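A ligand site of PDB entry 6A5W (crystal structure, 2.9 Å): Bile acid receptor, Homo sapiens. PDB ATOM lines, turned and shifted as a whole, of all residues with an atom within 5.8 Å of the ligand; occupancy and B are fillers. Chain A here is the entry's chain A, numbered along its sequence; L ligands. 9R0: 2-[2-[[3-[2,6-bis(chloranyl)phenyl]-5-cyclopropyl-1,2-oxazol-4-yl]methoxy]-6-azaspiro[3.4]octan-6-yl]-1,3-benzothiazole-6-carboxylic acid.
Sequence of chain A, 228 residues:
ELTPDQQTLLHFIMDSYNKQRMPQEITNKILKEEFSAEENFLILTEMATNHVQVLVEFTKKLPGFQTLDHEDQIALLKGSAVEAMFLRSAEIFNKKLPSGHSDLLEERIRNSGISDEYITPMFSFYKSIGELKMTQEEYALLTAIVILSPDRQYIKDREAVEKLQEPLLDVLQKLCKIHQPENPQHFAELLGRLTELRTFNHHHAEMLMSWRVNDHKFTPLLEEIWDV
A nitrogen (N1) of the ligand sits at hydrogen-bond distance from a ring nitrogen (NE2) of His 204 (3.3 Å).
An oxygen (O3) of the ligand lies within hydrogen-bond range of a ring nitrogen (ND1) of His 101 (2.8 Å).
OG of Ser 89 is in hydrogen-bond range of OH of Tyr 126 (2.8 Å).
The side-chain hydroxyl (OG1) of Thr 45 lies within hydrogen-bond range of the backbone carbonyl oxygen (O) of Phe 41 (2.9 Å).
OG of Ser 89 is in hydrogen-bond range of O of Phe 86, at 3.0 Å.
The side-chain sulfur (SD) of Met 122 lies close to the side-chain hydroxyl (OH) of Tyr 126, 3.6 Å away.
Residues that only touch the ligand: Trp 211 (3.2 Å), Phe 86 (3.3 Å), Met 47 (3.3 Å), Met 85 (3.4 Å), Ser 89 (3.4 Å), Ile 92 (3.4 Å), Leu 44 (3.5 Å), Thr 45 (3.5 Å), Trp 226 (3.6 Å), Phe 218 (3.6 Å), Ile 30 (3.6 Å), Thr 27 (3.6 Å), Ala 48 (3.6 Å), Tyr 126 (3.7 Å), Leu 105 (3.7 Å), Met 22 (3.8 Å), Leu 97 (3.8 Å), Pro 98 (3.9 Å), Met 207 (3.9 Å), Arg 88 (3.9 Å), Phe 41 (3.9 Å) and His 51 (3.9 Å).
Hydrophobic or aromatic side chains that line the ligand: Met 22, Ile 30, Phe 41, Leu 44, Met 47, Ala 48, His 51, Met 85, Phe 86, Ile 92, Leu 97, Pro 98, His 101, Leu 105, His 204, Met 207, Trp 211, Phe 218 and Trp 226.
The nearest printed residue that does not touch the ligand is Ile 114 (4.3 Å).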
ATOM      1  N   MET A  22     -13.480 -22.651  12.947  1.00  0.00           N
ATOM      2  CA  MET A  22     -14.865 -22.246  13.189  1.00  0.00           C
ATOM      3  C   MET A  22     -15.618 -23.544  13.422  1.00  0.00           C
ATOM      4  O   MET A  22     -15.573 -24.434  12.569  1.00  0.00           O
ATOM      5  CB  MET A  22     -15.475 -21.467  12.017  1.00  0.00           C
ATOM      6  CG  MET A  22     -16.863 -20.932  12.308  1.00  0.00           C
ATOM      7  SD  MET A  22     -16.973 -19.181  12.640  1.00  0.00           S
ATOM      8  CE  MET A  22     -15.547 -18.951  13.734  1.00  0.00           C
ATOM      9  N   THR A  27     -20.682 -23.436  11.095  1.00  0.00           N
ATOM     10  CA  THR A  27     -20.584 -23.526   9.621  1.00  0.00           C
ATOM     11  C   THR A  27     -21.791 -24.200   8.988  1.00  0.00           C
ATOM     12  O   THR A  27     -22.174 -23.872   7.861  1.00  0.00           O
ATOM     13  CB  THR A  27     -19.296 -24.255   9.087  1.00  0.00           C
ATOM     14  OG1 THR A  27     -19.293 -25.637   9.475  1.00  0.00           O
ATOM     15  CG2 THR A  27     -18.038 -23.573   9.548  1.00  0.00           C
ATOM     16  N   ILE A  30     -24.683 -22.007   7.545  1.00  0.00           N
ATOM     17  CA  ILE A  30     -24.545 -21.320   6.271  1.00  0.00           C
ATOM     18  C   ILE A  30     -25.554 -21.903   5.276  1.00  0.00           C
ATOM     19  O   ILE A  30     -26.305 -21.171   4.627  1.00  0.00           O
ATOM     20  CB  ILE A  30     -23.097 -21.419   5.735  1.00  0.00           C
ATOM     21  CG1 ILE A  30     -22.121 -20.656   6.650  1.00  0.00           C
ATOM     22  CG2 ILE A  30     -23.009 -20.857   4.336  1.00  0.00           C
ATOM     23  CD1 ILE A  30     -20.677 -21.018   6.424  1.00  0.00           C
ATOM     24  N   PHE A  41     -27.926 -11.898   9.804  1.00  0.00           N
ATOM     25  CA  PHE A  41     -27.230 -11.067  10.762  1.00  0.00           C
ATOM     26  C   PHE A  41     -26.812 -11.862  11.995  1.00  0.00           C
ATOM     27  O   PHE A  41     -25.682 -11.707  12.499  1.00  0.00           O
ATOM     28  CB  PHE A  41     -28.077  -9.871  11.168  1.00  0.00           C
ATOM     29  CG  PHE A  41     -27.447  -9.050  12.255  1.00  0.00           C
ATOM     30  CD1 PHE A  41     -26.376  -8.257  11.981  1.00  0.00           C
ATOM     31  CD2 PHE A  41     -27.866  -9.142  13.561  1.00  0.00           C
ATOM     32  CE1 PHE A  41     -25.756  -7.543  12.970  1.00  0.00           C
ATOM     33  CE2 PHE A  41     -27.255  -8.424  14.560  1.00  0.00           C
ATOM     34  CZ  PHE A  41     -26.201  -7.615  14.256  1.00  0.00           C
ATOM     35  N   LEU A  44     -23.895 -14.246  11.218  1.00  0.00           N
ATOM     36  CA  LEU A  44     -22.663 -13.481  11.288  1.00  0.00           C
ATOM     37  C   LEU A  44     -22.280 -13.104  12.722  1.00  0.00           C
ATOM     38  O   LEU A  44     -21.100 -13.156  13.070  1.00  0.00           O
ATOM     39  CB  LEU A  44     -22.764 -12.219  10.439  1.00  0.00           C
ATOM     40  CG  LEU A  44     -22.893 -12.429   8.926  1.00  0.00           C
ATOM     41  CD1 LEU A  44     -23.167 -11.076   8.303  1.00  0.00           C
ATOM     42  CD2 LEU A  44     -21.668 -13.050   8.280  1.00  0.00           C
ATOM     43  N   THR A  45     -23.244 -12.722  13.562  1.00  0.00           N
ATOM     44  CA  THR A  45     -22.923 -12.401  14.952  1.00  0.00           C
ATOM     45  C   THR A  45     -22.233 -13.580  15.693  1.00  0.00           C
ATOM     46  O   THR A  45     -21.259 -13.368  16.439  1.00  0.00           O
ATOM     47  CB  THR A  45     -24.140 -11.869  15.713  1.00  0.00           C
ATOM     48  OG1 THR A  45     -24.661 -10.728  15.026  1.00  0.00           O
ATOM     49  CG2 THR A  45     -23.757 -11.415  17.072  1.00  0.00           C
ATOM     50  N   MET A  47     -20.561 -16.095  14.187  1.00  0.00           N
ATOM     51  CA  MET A  47     -19.313 -16.231  13.489  1.00  0.00           C
ATOM     52  C   MET A  47     -18.274 -15.235  14.057  1.00  0.00           C
ATOM     53  O   MET A  47     -17.182 -15.653  14.437  1.00  0.00           O
ATOM     54  CB  MET A  47     -19.571 -16.078  11.999  1.00  0.00           C
ATOM     55  CG  MET A  47     -20.178 -17.349  11.438  1.00  0.00           C
ATOM     56  SD  MET A  47     -20.594 -17.469   9.691  1.00  0.00           S
ATOM     57  CE  MET A  47     -19.538 -16.227   9.024  1.00  0.00           C
ATOM     58  N   ALA A  48     -18.662 -13.963  14.197  1.00  0.00           N
ATOM     59  CA  ALA A  48     -17.824 -12.918  14.795  1.00  0.00           C
ATOM     60  C   ALA A  48     -17.359 -13.224  16.199  1.00  0.00           C
ATOM     61  O   ALA A  48     -16.181 -13.043  16.514  1.00  0.00           O
ATOM     62  CB  ALA A  48     -18.579 -11.602  14.852  1.00  0.00           C
ATOM     63  N   HIS A  51     -14.963 -16.144  16.348  1.00  0.00           N
ATOM     64  CA  HIS A  51     -13.654 -15.772  15.817  1.00  0.00           C
ATOM     65  C   HIS A  51     -12.893 -14.862  16.765  1.00  0.00           C
ATOM     66  O   HIS A  51     -11.680 -15.026  16.899  1.00  0.00           O
ATOM     67  CB  HIS A  51     -13.730 -15.125  14.430  1.00  0.00           C
ATOM     68  CG  HIS A  51     -12.376 -14.803  13.867  1.00  0.00           C
ATOM     69  ND1 HIS A  51     -11.517 -15.777  13.414  1.00  0.00           N
ATOM     70  CD2 HIS A  51     -11.723 -13.632  13.757  1.00  0.00           C
ATOM     71  CE1 HIS A  51     -10.383 -15.217  13.034  1.00  0.00           C
ATOM     72  NE2 HIS A  51     -10.487 -13.913  13.206  1.00  0.00           N
ATOM     73  N   VAL A  82     -10.434  -5.241  13.855  1.00  0.00           N
ATOM     74  CA  VAL A  82     -11.138  -5.090  12.606  1.00  0.00           C
ATOM     75  C   VAL A  82     -10.245  -5.532  11.483  1.00  0.00           C
ATOM     76  O   VAL A  82     -10.663  -6.268  10.600  1.00  0.00           O
ATOM     77  CB  VAL A  82     -11.623  -3.662  12.384  1.00  0.00           C
ATOM     78  CG1 VAL A  82     -12.111  -3.475  10.962  1.00  0.00           C
ATOM     79  CG2 VAL A  82     -12.752  -3.333  13.351  1.00  0.00           C
ATOM     80  N   MET A  85      -9.718  -9.299  11.462  1.00  0.00           N
ATOM     81  CA  MET A  85     -10.976  -9.939  11.074  1.00  0.00           C
ATOM     82  C   MET A  85     -11.197  -9.881   9.570  1.00  0.00           C
ATOM     83  O   MET A  85     -11.527 -10.897   8.968  1.00  0.00           O
ATOM     84  CB  MET A  85     -12.169  -9.372  11.863  1.00  0.00           C
ATOM     85  CG  MET A  85     -12.168  -9.834  13.315  1.00  0.00           C
ATOM     86  SD  MET A  85     -13.538  -9.347  14.376  1.00  0.00           S
ATOM     87  CE  MET A  85     -14.766 -10.496  13.774  1.00  0.00           C
ATOM     88  N   PHE A  86     -10.993  -8.717   8.964  1.00  0.00           N
ATOM     89  CA  PHE A  86     -11.169  -8.617   7.495  1.00  0.00           C
ATOM     90  C   PHE A  86     -10.105  -9.410   6.721  1.00  0.00           C
ATOM     91  O   PHE A  86     -10.386  -9.921   5.655  1.00  0.00           O
ATOM     92  CB  PHE A  86     -11.261  -7.170   7.017  1.00  0.00           C
ATOM     93  CG  PHE A  86     -12.633  -6.566   7.182  1.00  0.00           C
ATOM     94  CD1 PHE A  86     -12.995  -5.951   8.378  1.00  0.00           C
ATOM     95  CD2 PHE A  86     -13.555  -6.613   6.162  1.00  0.00           C
ATOM     96  CE1 PHE A  86     -14.250  -5.379   8.550  1.00  0.00           C
ATOM     97  CE2 PHE A  86     -14.825  -6.030   6.317  1.00  0.00           C
ATOM     98  CZ  PHE A  86     -15.166  -5.408   7.519  1.00  0.00           C
ATOM     99  N   ARG A  88      -8.775 -12.219   7.841  1.00  0.00           N
ATOM    100  CA  ARG A  88      -9.226 -13.592   7.956  1.00  0.00           C
ATOM    101  C   ARG A  88     -10.322 -13.856   6.909  1.00  0.00           C
ATOM    102  O   ARG A  88     -10.208 -14.788   6.121  1.00  0.00           O
ATOM    103  CB  ARG A  88      -9.764 -13.908   9.344  1.00  0.00           C
ATOM    104  CG  ARG A  88      -9.594 -15.355   9.822  1.00  0.00           C
ATOM    105  CD  ARG A  88      -9.674 -16.451   8.757  1.00  0.00           C
ATOM    106  NE  ARG A  88      -9.022 -17.719   9.148  1.00  0.00           N
ATOM    107  CZ  ARG A  88      -9.573 -18.660   9.887  1.00  0.00           C
ATOM    108  NH1 ARG A  88     -10.812 -18.547  10.388  1.00  0.00           N
ATOM    109  NH2 ARG A  88      -8.866 -19.757  10.139  1.00  0.00           N
ATOM    110  N   SER A  89     -11.358 -13.019   6.888  1.00  0.00           N
ATOM    111  CA  SER A  89     -12.463 -13.271   5.944  1.00  0.00           C
ATOM    112  C   SER A  89     -11.941 -13.294   4.516  1.00  0.00           C
ATOM    113  O   SER A  89     -12.439 -14.052   3.716  1.00  0.00           O
ATOM    114  CB  SER A  89     -13.629 -12.289   6.089  1.00  0.00           C
ATOM    115  OG  SER A  89     -13.194 -10.960   5.859  1.00  0.00           O
ATOM    116  N   ILE A  92     -10.612 -16.697   3.914  1.00  0.00           N
ATOM    117  CA  ILE A  92     -11.762 -17.593   3.796  1.00  0.00           C
ATOM    118  C   ILE A  92     -12.451 -17.505   2.427  1.00  0.00           C
ATOM    119  O   ILE A  92     -12.889 -18.519   1.876  1.00  0.00           O
ATOM    120  CB  ILE A  92     -12.765 -17.316   4.949  1.00  0.00           C
ATOM    121  CG1 ILE A  92     -12.167 -17.748   6.290  1.00  0.00           C
ATOM    122  CG2 ILE A  92     -14.151 -17.934   4.713  1.00  0.00           C
ATOM    123  CD1 ILE A  92     -11.984 -19.237   6.475  1.00  0.00           C
ATOM    124  N   LEU A  97     -13.811 -24.084   0.404  1.00  0.00           N
ATOM    125  CA  LEU A  97     -14.692 -24.428   1.531  1.00  0.00           C
ATOM    126  C   LEU A  97     -15.611 -25.527   1.007  1.00  0.00           C
ATOM    127  O   LEU A  97     -15.696 -25.716  -0.185  1.00  0.00           O
ATOM    128  CB  LEU A  97     -15.539 -23.214   1.950  1.00  0.00           C
ATOM    129  CG  LEU A  97     -14.845 -21.854   2.236  1.00  0.00           C
ATOM    130  CD1 LEU A  97     -15.828 -20.686   2.291  1.00  0.00           C
ATOM    131  CD2 LEU A  97     -14.066 -21.942   3.528  1.00  0.00           C
ATOM    132  N   PRO A  98     -16.325 -26.237   1.893  1.00  0.00           N
ATOM    133  CA  PRO A  98     -17.295 -27.238   1.416  1.00  0.00           C
ATOM    134  C   PRO A  98     -18.316 -26.702   0.397  1.00  0.00           C
ATOM    135  O   PRO A  98     -18.521 -25.493   0.311  1.00  0.00           O
ATOM    136  CB  PRO A  98     -18.003 -27.651   2.708  1.00  0.00           C
ATOM    137  CG  PRO A  98     -17.028 -27.390   3.806  1.00  0.00           C
ATOM    138  CD  PRO A  98     -16.249 -26.186   3.367  1.00  0.00           C
ATOM    139  N   HIS A 101     -20.776 -23.267   0.343  1.00  0.00           N
ATOM    140  CA  HIS A 101     -20.499 -22.418   1.491  1.00  0.00           C
ATOM    141  C   HIS A 101     -20.031 -21.051   1.025  1.00  0.00           C
ATOM    142  O   HIS A 101     -20.590 -20.021   1.438  1.00  0.00           O
ATOM    143  CB  HIS A 101     -19.436 -23.022   2.405  1.00  0.00           C
ATOM    144  CG  HIS A 101     -19.922 -24.144   3.265  1.00  0.00           C
ATOM    145  ND1 HIS A 101     -19.353 -24.440   4.495  1.00  0.00           N
ATOM    146  CD2 HIS A 101     -20.918 -25.041   3.088  1.00  0.00           C
ATOM    147  CE1 HIS A 101     -19.969 -25.481   5.028  1.00  0.00           C
ATOM    148  NE2 HIS A 101     -20.931 -25.863   4.198  1.00  0.00           N
ATOM    149  N   LEU A 105     -22.570 -18.012   1.864  1.00  0.00           N
ATOM    150  CA  LEU A 105     -22.046 -17.105   2.877  1.00  0.00           C
ATOM    151  C   LEU A 105     -22.022 -15.695   2.328  1.00  0.00           C
ATOM    152  O   LEU A 105     -22.393 -14.739   3.029  1.00  0.00           O
ATOM    153  CB  LEU A 105     -20.647 -17.506   3.295  1.00  0.00           C
ATOM    154  CG  LEU A 105     -19.965 -16.603   4.322  1.00  0.00           C
ATOM    155  CD1 LEU A 105     -20.845 -16.334   5.517  1.00  0.00           C
ATOM    156  CD2 LEU A 105     -18.653 -17.202   4.763  1.00  0.00           C
ATOM    157  N   ILE A 109     -24.004 -12.357   3.694  1.00  0.00           N
ATOM    158  CA  ILE A 109     -23.368 -11.058   3.980  1.00  0.00           C
ATOM    159  C   ILE A 109     -24.007  -9.941   3.188  1.00  0.00           C
ATOM    160  O   ILE A 109     -24.239  -8.819   3.681  1.00  0.00           O
ATOM    161  CB  ILE A 109     -21.877 -11.141   3.689  1.00  0.00           C
ATOM    162  CG1 ILE A 109     -21.234 -11.962   4.797  1.00  0.00           C
ATOM    163  CG2 ILE A 109     -21.236  -9.782   3.647  1.00  0.00           C
ATOM    164  CD1 ILE A 109     -19.879 -12.483   4.434  1.00  0.00           C
ATOM    165  N   ILE A 114     -26.027  -4.716   5.599  1.00  0.00           N
ATOM    166  CA  ILE A 114     -24.794  -3.954   5.322  1.00  0.00           C
ATOM    167  C   ILE A 114     -25.014  -3.169   4.041  1.00  0.00           C
ATOM    168  O   ILE A 114     -25.260  -3.770   3.009  1.00  0.00           O
ATOM    169  CB  ILE A 114     -23.560  -4.852   5.129  1.00  0.00           C
ATOM    170  CG1 ILE A 114     -23.287  -5.704   6.373  1.00  0.00           C
ATOM    171  CG2 ILE A 114     -22.323  -4.001   4.834  1.00  0.00           C
ATOM    172  CD1 ILE A 114     -22.373  -6.883   6.087  1.00  0.00           C
ATOM    173  N   MET A 122     -15.539  -4.255   0.390  1.00  0.00           N
ATOM    174  CA  MET A 122     -15.317  -5.547   1.034  1.00  0.00           C
ATOM    175  C   MET A 122     -14.939  -6.618   0.011  1.00  0.00           C
ATOM    176  O   MET A 122     -13.886  -7.245   0.139  1.00  0.00           O
ATOM    177  CB  MET A 122     -16.551  -5.965   1.860  1.00  0.00           C
ATOM    178  CG  MET A 122     -16.410  -7.310   2.578  1.00  0.00           C
ATOM    179  SD  MET A 122     -17.944  -7.875   3.378  1.00  0.00           S
ATOM    180  CE  MET A 122     -18.339  -6.419   4.349  1.00  0.00           C
ATOM    181  N   TYR A 126     -11.346  -8.566  -1.173  1.00  0.00           N
ATOM    182  CA  TYR A 126     -11.164 -10.027  -1.242  1.00  0.00           C
ATOM    183  C   TYR A 126     -10.622 -10.475  -2.601  1.00  0.00           C
ATOM    184  O   TYR A 126      -9.861 -11.434  -2.670  1.00  0.00           O
ATOM    185  CB  TYR A 126     -12.459 -10.804  -0.935  1.00  0.00           C
ATOM    186  CG  TYR A 126     -13.128 -10.555   0.402  1.00  0.00           C
ATOM    187  CD1 TYR A 126     -12.405 -10.299   1.554  1.00  0.00           C
ATOM    188  CD2 TYR A 126     -14.484 -10.647   0.523  1.00  0.00           C
ATOM    189  CE1 TYR A 126     -13.046 -10.107   2.771  1.00  0.00           C
ATOM    190  CE2 TYR A 126     -15.136 -10.447   1.737  1.00  0.00           C
ATOM    191  CZ  TYR A 126     -14.409 -10.187   2.852  1.00  0.00           C
ATOM    192  OH  TYR A 126     -15.075  -9.980   4.033  1.00  0.00           O
ATOM    193  N   HIS A 204     -16.046  -0.697   8.677  1.00  0.00           N
ATOM    194  CA  HIS A 204     -16.637  -1.432   9.796  1.00  0.00           C
ATOM    195  C   HIS A 204     -17.292  -0.531  10.879  1.00  0.00           C
ATOM    196  O   HIS A 204     -18.322  -0.893  11.466  1.00  0.00           O
ATOM    197  CB  HIS A 204     -15.597  -2.334  10.436  1.00  0.00           C
ATOM    198  CG  HIS A 204     -16.196  -3.300  11.395  1.00  0.00           C
ATOM    199  ND1 HIS A 204     -16.108  -3.137  12.743  1.00  0.00           N
ATOM    200  CD2 HIS A 204     -16.962  -4.397  11.188  1.00  0.00           C
ATOM    201  CE1 HIS A 204     -16.755  -4.122  13.337  1.00  0.00           C
ATOM    202  NE2 HIS A 204     -17.300  -4.890  12.423  1.00  0.00           N
ATOM    203  N   MET A 207     -20.462   0.308   9.434  1.00  0.00           N
ATOM    204  CA  MET A 207     -21.300  -0.898   9.425  1.00  0.00           C
ATOM    205  C   MET A 207     -22.044  -1.081  10.742  1.00  0.00           C
ATOM    206  O   MET A 207     -23.225  -1.425  10.754  1.00  0.00           O
ATOM    207  CB  MET A 207     -20.473  -2.127   9.111  1.00  0.00           C
ATOM    208  CG  MET A 207     -20.125  -2.234   7.637  1.00  0.00           C
ATOM    209  SD  MET A 207     -18.856  -3.453   7.355  1.00  0.00           S
ATOM    210  CE  MET A 207     -19.628  -4.860   8.114  1.00  0.00           C
ATOM    211  N   LEU A 208     -21.319  -0.835  11.830  1.00  0.00           N
ATOM    212  CA  LEU A 208     -21.869  -0.860  13.174  1.00  0.00           C
ATOM    213  C   LEU A 208     -22.802   0.289  13.454  1.00  0.00           C
ATOM    214  O   LEU A 208     -23.812   0.092  14.087  1.00  0.00           O
ATOM    215  CB  LEU A 208     -20.760  -0.792  14.233  1.00  0.00           C
ATOM    216  CG  LEU A 208     -19.768  -1.939  14.401  1.00  0.00           C
ATOM    217  CD1 LEU A 208     -18.953  -1.721  15.667  1.00  0.00           C
ATOM    218  CD2 LEU A 208     -20.490  -3.270  14.460  1.00  0.00           C
ATOM    219  N   TRP A 211     -26.070  -0.574  11.731  1.00  0.00           N
ATOM    220  CA  TRP A 211     -26.665  -1.673  12.468  1.00  0.00           C
ATOM    221  C   TRP A 211     -27.299  -1.200  13.777  1.00  0.00           C
ATOM    222  O   TRP A 211     -28.410  -1.601  14.074  1.00  0.00           O
ATOM    223  CB  TRP A 211     -25.614  -2.736  12.756  1.00  0.00           C
ATOM    224  CG  TRP A 211     -25.453  -3.759  11.720  1.00  0.00           C
ATOM    225  CD1 TRP A 211     -26.419  -4.281  10.916  1.00  0.00           C
ATOM    226  CD2 TRP A 211     -24.258  -4.483  11.424  1.00  0.00           C
ATOM    227  NE1 TRP A 211     -25.899  -5.279  10.136  1.00  0.00           N
ATOM    228  CE2 TRP A 211     -24.576  -5.429  10.420  1.00  0.00           C
ATOM    229  CE3 TRP A 211     -22.948  -4.434  11.898  1.00  0.00           C
ATOM    230  CZ2 TRP A 211     -23.641  -6.306   9.892  1.00  0.00           C
ATOM    231  CZ3 TRP A 211     -22.025  -5.303  11.368  1.00  0.00           C
ATOM    232  CH2 TRP A 211     -22.376  -6.244  10.371  1.00  0.00           C
ATOM    233  N   PHE A 218     -25.441  -7.024  19.562  1.00  0.00           N
ATOM    234  CA  PHE A 218     -24.262  -7.883  19.415  1.00  0.00           C
ATOM    235  C   PHE A 218     -24.016  -8.589  20.700  1.00  0.00           C
ATOM    236  O   PHE A 218     -24.455  -8.110  21.741  1.00  0.00           O
ATOM    237  CB  PHE A 218     -23.036  -7.028  19.070  1.00  0.00           C
ATOM    238  CG  PHE A 218     -23.252  -6.142  17.895  1.00  0.00           C
ATOM    239  CD1 PHE A 218     -23.041  -6.622  16.626  1.00  0.00           C
ATOM    240  CD2 PHE A 218     -23.733  -4.867  18.068  1.00  0.00           C
ATOM    241  CE1 PHE A 218     -23.293  -5.834  15.540  1.00  0.00           C
ATOM    242  CE2 PHE A 218     -23.972  -4.073  16.981  1.00  0.00           C
ATOM    243  CZ  PHE A 218     -23.765  -4.562  15.703  1.00  0.00           C
ATOM    244  N   LEU A 222     -18.294  -8.979  21.614  1.00  0.00           N
ATOM    245  CA  LEU A 222     -18.159  -8.089  20.472  1.00  0.00           C
ATOM    246  C   LEU A 222     -18.312  -6.670  20.920  1.00  0.00           C
ATOM    247  O   LEU A 222     -17.589  -5.802  20.442  1.00  0.00           O
ATOM    248  CB  LEU A 222     -19.202  -8.353  19.392  1.00  0.00           C
ATOM    249  CG  LEU A 222     -19.156  -9.745  18.754  1.00  0.00           C
ATOM    250  CD1 LEU A 222     -20.314  -9.904  17.781  1.00  0.00           C
ATOM    251  CD2 LEU A 222     -17.827 -10.021  18.088  1.00  0.00           C
ATOM    252  N   TRP A 226     -15.068  -4.130  20.194  1.00  0.00           N
ATOM    253  CA  TRP A 226     -15.416  -3.036  19.257  1.00  0.00           C
ATOM    254  C   TRP A 226     -15.850  -1.683  19.881  1.00  0.00           C
ATOM    255  O   TRP A 226     -16.289  -0.845  19.109  1.00  0.00           O
ATOM    256  CB  TRP A 226     -16.520  -3.513  18.267  1.00  0.00           C
ATOM    257  CG  TRP A 226     -16.128  -4.621  17.327  1.00  0.00           C
ATOM    258  CD1 TRP A 226     -14.874  -4.962  16.919  1.00  0.00           C
ATOM    259  CD2 TRP A 226     -17.026  -5.513  16.652  1.00  0.00           C
ATOM    260  NE1 TRP A 226     -14.932  -6.022  16.026  1.00  0.00           N
ATOM    261  CE2 TRP A 226     -16.243  -6.374  15.850  1.00  0.00           C
ATOM    262  CE3 TRP A 226     -18.409  -5.660  16.642  1.00  0.00           C
ATOM    263  CZ2 TRP A 226     -16.806  -7.359  15.052  1.00  0.00           C
ATOM    264  CZ3 TRP A 226     -18.965  -6.644  15.851  1.00  0.00           C
ATOM    265  CH2 TRP A 226     -18.169  -7.481  15.061  1.00  0.00           C
HETATM  266  C1  9R0 L   1     -16.576  -9.219   7.338  1.00  0.00           C
HETATM  267  C2  9R0 L   1     -17.567  -9.055   8.288  1.00  0.00           C
HETATM  268  C3  9R0 L   1     -17.285  -8.708   9.597  1.00  0.00           C
HETATM  269  C4  9R0 L   1     -15.970  -8.533   9.936  1.00  0.00           C
HETATM  270  C5  9R0 L   1     -14.955  -8.695   9.004  1.00  0.00           C
HETATM  271  C6  9R0 L   1     -15.263  -9.035   7.710  1.00  0.00           C
HETATM  272  C7  9R0 L   1     -18.366  -8.580  10.598  1.00  0.00           C
HETATM  273  N1  9R0 L   1     -18.791  -7.391  10.968  1.00  0.00           N
HETATM  274  O1  9R0 L   1     -19.822  -7.628  11.916  1.00  0.00           O
HETATM  275  C8  9R0 L   1     -19.949  -8.955  12.074  1.00  0.00           C
HETATM  276  C9  9R0 L   1     -19.087  -9.550  11.278  1.00  0.00           C
HETATM  277  C10 9R0 L   1     -20.942  -9.480  13.002  1.00  0.00           C
HETATM  278  C11 9R0 L   1     -22.372  -9.483  12.572  1.00  0.00           C
HETATM  279  C12 9R0 L   1     -21.914  -8.534  13.610  1.00  0.00           C
HETATM  280  C13 9R0 L   1     -18.948 -11.016  11.231  1.00  0.00           C
HETATM  281  O2  9R0 L   1     -18.096 -11.524  10.231  1.00  0.00           O
HETATM  282  C14 9R0 L   1     -16.836 -12.036  10.596  1.00  0.00           C
HETATM  283  C15 9R0 L   1     -16.827 -13.470  11.094  1.00  0.00           C
HETATM  284  C16 9R0 L   1     -15.772 -13.853  10.004  1.00  0.00           C
HETATM  285  C17 9R0 L   1     -15.965 -12.436   9.400  1.00  0.00           C
HETATM  286  C18 9R0 L   1     -16.154 -14.946   9.034  1.00  0.00           C
HETATM  287  N2  9R0 L   1     -15.187 -15.995   9.312  1.00  0.00           N
HETATM  288  C19 9R0 L   1     -13.971 -15.496   9.897  1.00  0.00           C
HETATM  289  C20 9R0 L   1     -14.369 -14.184  10.547  1.00  0.00           C
HETATM  290  C21 9R0 L   1     -15.391 -17.309   8.933  1.00  0.00           C
HETATM  291  N3  9R0 L   1     -14.544 -18.282   9.234  1.00  0.00           N
HETATM  292  C22 9R0 L   1     -14.922 -19.439   8.552  1.00  0.00           C
HETATM  293  C23 9R0 L   1     -16.103 -19.336   7.807  1.00  0.00           C
HETATM  294  S1  9R0 L   1     -16.756 -17.730   7.919  1.00  0.00           S
HETATM  295  C24 9R0 L   1     -14.240 -20.658   8.554  1.00  0.00           C
HETATM  296  C25 9R0 L   1     -14.747 -21.722   7.842  1.00  0.00           C
HETATM  297  C26 9R0 L   1     -15.934 -21.625   7.104  1.00  0.00           C
HETATM  298  C27 9R0 L   1     -16.619 -20.401   7.089  1.00  0.00           C
HETATM  299  C28 9R0 L   1     -16.534 -22.798   6.331  1.00  0.00           C
HETATM  300  O3  9R0 L   1     -17.532 -22.567   5.613  1.00  0.00           O
HETATM  301  O4  9R0 L   1     -16.039 -23.934   6.498  1.00  0.00           O
HETATM  302 CL1  9R0 L   1     -19.204  -9.258   7.806  1.00  0.00          CL
HETATM  303 CL2  9R0 L   1     -15.552  -8.109  11.558  1.00  0.00          CL
